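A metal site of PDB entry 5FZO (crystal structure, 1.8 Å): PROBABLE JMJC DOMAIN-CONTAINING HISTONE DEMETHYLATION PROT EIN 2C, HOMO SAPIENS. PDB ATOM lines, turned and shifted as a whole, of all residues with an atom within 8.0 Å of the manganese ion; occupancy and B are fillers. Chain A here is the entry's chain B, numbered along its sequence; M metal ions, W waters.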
ATOM      1  N   ARG A 160       8.012  -6.170 -23.031  1.00  0.00           N
ATOM      2  CA  ARG A 160       7.679  -6.917 -21.821  1.00  0.00           C
ATOM      3  C   ARG A 160       7.171  -5.951 -20.754  1.00  0.00           C
ATOM      4  O   ARG A 160       7.749  -4.889 -20.550  1.00  0.00           O
ATOM      5  CB  ARG A 160       8.895  -7.672 -21.264  1.00  0.00           C
ATOM      6  CG  ARG A 160       9.526  -8.670 -22.192  1.00  0.00           C
ATOM      7  CD  ARG A 160      10.816  -9.210 -21.620  1.00  0.00           C
ATOM      8  NE  ARG A 160      11.908  -8.238 -21.655  1.00  0.00           N
ATOM      9  CZ  ARG A 160      12.636  -7.971 -22.733  1.00  0.00           C
ATOM     10  NH1 ARG A 160      12.391  -8.598 -23.872  1.00  0.00           N
ATOM     11  NH2 ARG A 160      13.611  -7.077 -22.673  1.00  0.00           N
ATOM     12  N   CSD A 162       6.747  -5.478 -16.715  1.00  0.00           N
ATOM     13  CA  CSD A 162       7.209  -5.987 -15.449  1.00  0.00           C
ATOM     14  CB  CSD A 162       8.743  -5.960 -15.361  1.00  0.00           C
ATOM     15  SG  CSD A 162       9.347  -7.253 -14.349  1.00  0.00           S
ATOM     16  C   CSD A 162       6.633  -5.135 -14.332  1.00  0.00           C
ATOM     17  O   CSD A 162       6.699  -3.915 -14.334  1.00  0.00           O
ATOM     18  OD1 CSD A 162      11.010  -7.001 -14.602  1.00  0.00           O
ATOM     19  OD2 CSD A 162       9.331  -6.714 -12.994  1.00  0.00           O
ATOM     20  N   THR A 178      14.851  -6.998  -9.272  1.00  0.00           N
ATOM     21  CA  THR A 178      15.510  -7.621 -10.419  1.00  0.00           C
ATOM     22  C   THR A 178      16.928  -7.975 -10.021  1.00  0.00           C
ATOM     23  O   THR A 178      17.719  -7.097  -9.679  1.00  0.00           O
ATOM     24  CB  THR A 178      15.516  -6.722 -11.665  1.00  0.00           C
ATOM     25  OG1 THR A 178      14.175  -6.391 -12.022  1.00  0.00           O
ATOM     26  CG2 THR A 178      16.177  -7.447 -12.822  1.00  0.00           C
ATOM     27  N   ASN A 179      17.247  -9.266 -10.005  1.00  0.00           N
ATOM     28  CA  ASN A 179      18.592  -9.652  -9.572  1.00  0.00           C
ATOM     29  C   ASN A 179      19.651  -9.269 -10.595  1.00  0.00           C
ATOM     30  O   ASN A 179      19.332  -9.020 -11.767  1.00  0.00           O
ATOM     31  CB  ASN A 179      18.640 -11.165  -9.299  1.00  0.00           C
ATOM     32  CG  ASN A 179      17.993 -11.551  -7.984  1.00  0.00           C
ATOM     33  OD1 ASN A 179      17.765 -10.715  -7.100  1.00  0.00           O
ATOM     34  ND2 ASN A 179      17.726 -12.837  -7.826  1.00  0.00           N
ATOM     35  N   HIS A 181      22.048  -9.350 -13.406  1.00  0.00           N
ATOM     36  CA  HIS A 181      22.005 -10.182 -14.593  1.00  0.00           C
ATOM     37  C   HIS A 181      22.545  -9.403 -15.775  1.00  0.00           C
ATOM     38  O   HIS A 181      22.705  -8.185 -15.704  1.00  0.00           O
ATOM     39  CB  HIS A 181      20.592 -10.654 -14.884  1.00  0.00           C
ATOM     40  CG  HIS A 181      19.701  -9.562 -15.381  1.00  0.00           C
ATOM     41  ND1 HIS A 181      19.301  -8.504 -14.585  1.00  0.00           N
ATOM     42  CD2 HIS A 181      19.158  -9.340 -16.598  1.00  0.00           C
ATOM     43  CE1 HIS A 181      18.542  -7.688 -15.292  1.00  0.00           C
ATOM     44  NE2 HIS A 181      18.445  -8.172 -16.519  1.00  0.00           N
ATOM     45  N   ILE A 182      22.802 -10.113 -16.871  1.00  0.00           N
ATOM     46  CA  ILE A 182      23.350  -9.484 -18.072  1.00  0.00           C
ATOM     47  C   ILE A 182      22.270  -9.309 -19.130  1.00  0.00           C
ATOM     48  O   ILE A 182      21.314 -10.088 -19.194  1.00  0.00           O
ATOM     49  CB  ILE A 182      24.531 -10.318 -18.637  1.00  0.00           C
ATOM     50  CG1 ILE A 182      25.464  -9.459 -19.489  1.00  0.00           C
ATOM     51  CG2 ILE A 182      24.027 -11.550 -19.388  1.00  0.00           C
ATOM     52  CD1 ILE A 182      26.728 -10.188 -19.910  1.00  0.00           C
ATOM     53  N   GLU A 183      22.419  -8.258 -19.940  1.00  0.00           N
ATOM     54  CA  GLU A 183      21.513  -7.982 -21.048  1.00  0.00           C
ATOM     55  C   GLU A 183      21.972  -8.652 -22.337  1.00  0.00           C
ATOM     56  O   GLU A 183      23.079  -8.401 -22.799  1.00  0.00           O
ATOM     57  CB  GLU A 183      21.377  -6.477 -21.287  1.00  0.00           C
ATOM     58  CG  GLU A 183      20.840  -5.666 -20.127  1.00  0.00           C
ATOM     59  CD  GLU A 183      19.403  -6.027 -19.758  1.00  0.00           C
ATOM     60  OE1 GLU A 183      18.753  -6.826 -20.476  1.00  0.00           O
ATOM     61  OE2 GLU A 183      18.920  -5.482 -18.727  1.00  0.00           O
ATOM     62  N   VAL A 184      21.123  -9.498 -22.907  1.00  0.00           N
ATOM     63  CA  VAL A 184      21.479 -10.212 -24.119  1.00  0.00           C
ATOM     64  C   VAL A 184      21.367  -9.317 -25.354  1.00  0.00           C
ATOM     65  O   VAL A 184      22.124  -9.473 -26.318  1.00  0.00           O
ATOM     66  CB  VAL A 184      20.603 -11.495 -24.252  1.00  0.00           C
ATOM     67  CG1 VAL A 184      19.991 -11.642 -25.619  1.00  0.00           C
ATOM     68  CG2 VAL A 184      21.413 -12.713 -23.846  1.00  0.00           C
ATOM     69  N   ASP A 185      20.473  -8.342 -25.318  1.00  0.00           N
ATOM     70  CA  ASP A 185      20.438  -7.355 -26.389  1.00  0.00           C
ATOM     71  C   ASP A 185      20.218  -5.940 -25.867  1.00  0.00           C
ATOM     72  O   ASP A 185      20.115  -5.714 -24.661  1.00  0.00           O
ATOM     73  CB  ASP A 185      19.364  -7.715 -27.398  1.00  0.00           C
ATOM     74  CG  ASP A 185      18.002  -7.318 -26.939  1.00  0.00           C
ATOM     75  OD1 ASP A 185      17.640  -7.667 -25.799  1.00  0.00           O
ATOM     76  OD2 ASP A 185      17.302  -6.660 -27.723  1.00  0.00           O
ATOM     77  N   VAL A 187      18.274  -2.746 -24.902  1.00  0.00           N
ATOM     78  CA  VAL A 187      16.964  -2.679 -24.305  1.00  0.00           C
ATOM     79  C   VAL A 187      16.689  -1.283 -23.737  1.00  0.00           C
ATOM     80  O   VAL A 187      17.602  -0.584 -23.297  1.00  0.00           O
ATOM     81  CB  VAL A 187      16.804  -3.746 -23.192  1.00  0.00           C
ATOM     82  CG1 VAL A 187      17.747  -3.463 -22.010  1.00  0.00           C
ATOM     83  CG2 VAL A 187      15.353  -3.831 -22.739  1.00  0.00           C
ATOM     84  N   ASN A 189      14.227   0.497 -20.884  1.00  0.00           N
ATOM     85  CA  ASN A 189      13.330   0.262 -19.748  1.00  0.00           C
ATOM     86  C   ASN A 189      12.664   1.549 -19.315  1.00  0.00           C
ATOM     87  O   ASN A 189      13.331   2.482 -18.874  1.00  0.00           O
ATOM     88  CB  ASN A 189      14.105  -0.342 -18.576  1.00  0.00           C
ATOM     89  CG  ASN A 189      13.197  -0.757 -17.428  1.00  0.00           C
ATOM     90  OD1 ASN A 189      12.563   0.077 -16.766  1.00  0.00           O
ATOM     91  ND2 ASN A 189      13.149  -2.054 -17.186  1.00  0.00           N
ATOM     92  N   TRP A 236      18.598   1.604  -9.121  1.00  0.00           N
ATOM     93  CA  TRP A 236      19.314   0.750 -10.073  1.00  0.00           C
ATOM     94  C   TRP A 236      20.794   0.745  -9.760  1.00  0.00           C
ATOM     95  O   TRP A 236      21.351   1.780  -9.419  1.00  0.00           O
ATOM     96  CB  TRP A 236      19.139   1.254 -11.510  1.00  0.00           C
ATOM     97  CG  TRP A 236      17.826   1.023 -12.112  1.00  0.00           C
ATOM     98  CD1 TRP A 236      16.621   1.477 -11.656  1.00  0.00           C
ATOM     99  CD2 TRP A 236      17.578   0.350 -13.338  1.00  0.00           C
ATOM    100  NE1 TRP A 236      15.625   1.088 -12.529  1.00  0.00           N
ATOM    101  CE2 TRP A 236      16.177   0.403 -13.566  1.00  0.00           C
ATOM    102  CE3 TRP A 236      18.382  -0.297 -14.266  1.00  0.00           C
ATOM    103  CZ2 TRP A 236      15.582  -0.198 -14.685  1.00  0.00           C
ATOM    104  CZ3 TRP A 236      17.793  -0.877 -15.384  1.00  0.00           C
ATOM    105  CH2 TRP A 236      16.395  -0.812 -15.583  1.00  0.00           C
ATOM    106  N   GLN A 272      21.397 -15.585 -12.248  1.00  0.00           N
ATOM    107  CA  GLN A 272      20.592 -14.429 -11.853  1.00  0.00           C
ATOM    108  C   GLN A 272      20.060 -14.629 -10.427  1.00  0.00           C
ATOM    109  O   GLN A 272      18.862 -14.433 -10.174  1.00  0.00           O
ATOM    110  CB  GLN A 272      19.438 -14.208 -12.821  1.00  0.00           C
ATOM    111  CG  GLN A 272      19.872 -14.179 -14.266  1.00  0.00           C
ATOM    112  CD  GLN A 272      18.758 -13.749 -15.189  1.00  0.00           C
ATOM    113  OE1 GLN A 272      17.746 -13.215 -14.750  1.00  0.00           O
ATOM    114  NE2 GLN A 272      18.950 -13.959 -16.490  1.00  0.00           N
ATOM    115  N   LEU A 305      20.079   0.529 -22.163  1.00  0.00           N
ATOM    116  CA  LEU A 305      21.265  -0.288 -21.896  1.00  0.00           C
ATOM    117  C   LEU A 305      21.705  -1.082 -23.120  1.00  0.00           C
ATOM    118  O   LEU A 305      20.873  -1.671 -23.826  1.00  0.00           O
ATOM    119  CB  LEU A 305      20.991  -1.254 -20.752  1.00  0.00           C
ATOM    120  CG  LEU A 305      20.539  -0.672 -19.411  1.00  0.00           C
ATOM    121  CD1 LEU A 305      20.144  -1.803 -18.465  1.00  0.00           C
ATOM    122  CD2 LEU A 305      21.654   0.143 -18.818  1.00  0.00           C
ATOM    123  N   ALA A 309      25.550  -5.076 -20.890  1.00  0.00           N
ATOM    124  CA  ALA A 309      25.549  -4.374 -19.611  1.00  0.00           C
ATOM    125  C   ALA A 309      24.967  -5.253 -18.525  1.00  0.00           C
ATOM    126  O   ALA A 309      24.072  -6.063 -18.782  1.00  0.00           O
ATOM    127  CB  ALA A 309      24.780  -3.043 -19.704  1.00  0.00           C
ATOM    128  N   LEU A 310      25.465  -5.103 -17.314  1.00  0.00           N
ATOM    129  CA  LEU A 310      24.893  -5.792 -16.161  1.00  0.00           C
ATOM    130  C   LEU A 310      24.168  -4.817 -15.260  1.00  0.00           C
ATOM    131  O   LEU A 310      24.618  -3.679 -15.068  1.00  0.00           O
ATOM    132  CB  LEU A 310      25.972  -6.515 -15.350  1.00  0.00           C
ATOM    133  CG  LEU A 310      26.663  -7.721 -15.976  1.00  0.00           C
ATOM    134  CD1 LEU A 310      28.023  -7.325 -16.543  1.00  0.00           C
ATOM    135  CD2 LEU A 310      26.784  -8.838 -14.935  1.00  0.00           C
ATOM    136  N   HIS A 311      23.047  -5.264 -14.698  1.00  0.00           N
ATOM    137  CA  HIS A 311      22.367  -4.470 -13.696  1.00  0.00           C
ATOM    138  C   HIS A 311      21.448  -5.275 -12.788  1.00  0.00           C
ATOM    139  O   HIS A 311      21.060  -6.408 -13.082  1.00  0.00           O
ATOM    140  CB  HIS A 311      21.578  -3.348 -14.381  1.00  0.00           C
ATOM    141  CG  HIS A 311      20.293  -3.809 -15.007  1.00  0.00           C
ATOM    142  ND1 HIS A 311      19.071  -3.646 -14.392  1.00  0.00           N
ATOM    143  CD2 HIS A 311      20.047  -4.420 -16.187  1.00  0.00           C
ATOM    144  CE1 HIS A 311      18.127  -4.134 -15.173  1.00  0.00           C
ATOM    145  NE2 HIS A 311      18.684  -4.594 -16.270  1.00  0.00           N
ATOM    146  N   GLN A 312      21.082  -4.632 -11.698  1.00  0.00           N
ATOM    147  CA  GLN A 312      20.095  -5.106 -10.770  1.00  0.00           C
ATOM    148  C   GLN A 312      19.183  -3.940 -10.432  1.00  0.00           C
ATOM    149  O   GLN A 312      19.535  -2.768 -10.659  1.00  0.00           O
ATOM    150  CB  GLN A 312      20.774  -5.655  -9.514  1.00  0.00           C
ATOM    151  CG  GLN A 312      21.648  -4.616  -8.814  1.00  0.00           C
ATOM    152  CD  GLN A 312      22.377  -5.200  -7.604  1.00  0.00           C
ATOM    153  OE1 GLN A 312      22.613  -6.400  -7.523  1.00  0.00           O
ATOM    154  NE2 GLN A 312      22.729  -4.333  -6.673  1.00  0.00           N
ATOM    155  N   VAL A 313      17.997  -4.253  -9.933  1.00  0.00           N
ATOM    156  CA  VAL A 313      17.026  -3.237  -9.581  1.00  0.00           C
ATOM    157  C   VAL A 313      16.383  -3.542  -8.227  1.00  0.00           C
ATOM    158  O   VAL A 313      16.158  -4.700  -7.879  1.00  0.00           O
ATOM    159  CB  VAL A 313      15.898  -3.095 -10.627  1.00  0.00           C
ATOM    160  CG1 VAL A 313      15.022  -1.887 -10.309  1.00  0.00           C
ATOM    161  CG2 VAL A 313      16.454  -2.964 -12.028  1.00  0.00           C
ATOM    162  N   THR A 323       9.616  -2.769 -21.045  1.00  0.00           N
ATOM    163  CA  THR A 323      10.938  -2.845 -21.634  1.00  0.00           C
ATOM    164  C   THR A 323      10.794  -3.273 -23.080  1.00  0.00           C
ATOM    165  O   THR A 323       9.955  -4.124 -23.420  1.00  0.00           O
ATOM    166  CB  THR A 323      11.881  -3.792 -20.876  1.00  0.00           C
ATOM    167  OG1 THR A 323      11.634  -5.147 -21.275  1.00  0.00           O
ATOM    168  CG2 THR A 323      11.669  -3.676 -19.414  1.00  0.00           C
HETATM  169 MN    MN M   1      17.379  -5.967 -17.423  1.00  0.00          MN
HETATM  170  O   HOH W   1      15.573  -4.496 -18.780  1.00  0.00           O
HETATM  171  O   HOH W   2      17.092  -7.818 -19.038  1.00  0.00           O
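The manganese ion is bound by the side-chain carboxylate of Glu 183 (2.1 Å), a ring nitrogen (NE2) of His 311 (2.2 Å), water W2 (2.5 Å), a ring nitrogen (NE2) of His 181 (2.6 Å) and water W1 (2.7 Å).
The manganese ion has five donor atoms within binding distance.
Of the 20 residues printed, 3 come within 4 Å of the manganese ion.
The nearest printed residue that does not touch the manganese ion is Thr 178 (5.0 Å).
The backbone carbonyl oxygen (O) of Asn 179 is in hydrogen-bond range of a ring nitrogen (ND1) of His 181 (2.9 Å).
N of Glu 183 sits at hydrogen-bond distance from O of Ala 309.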
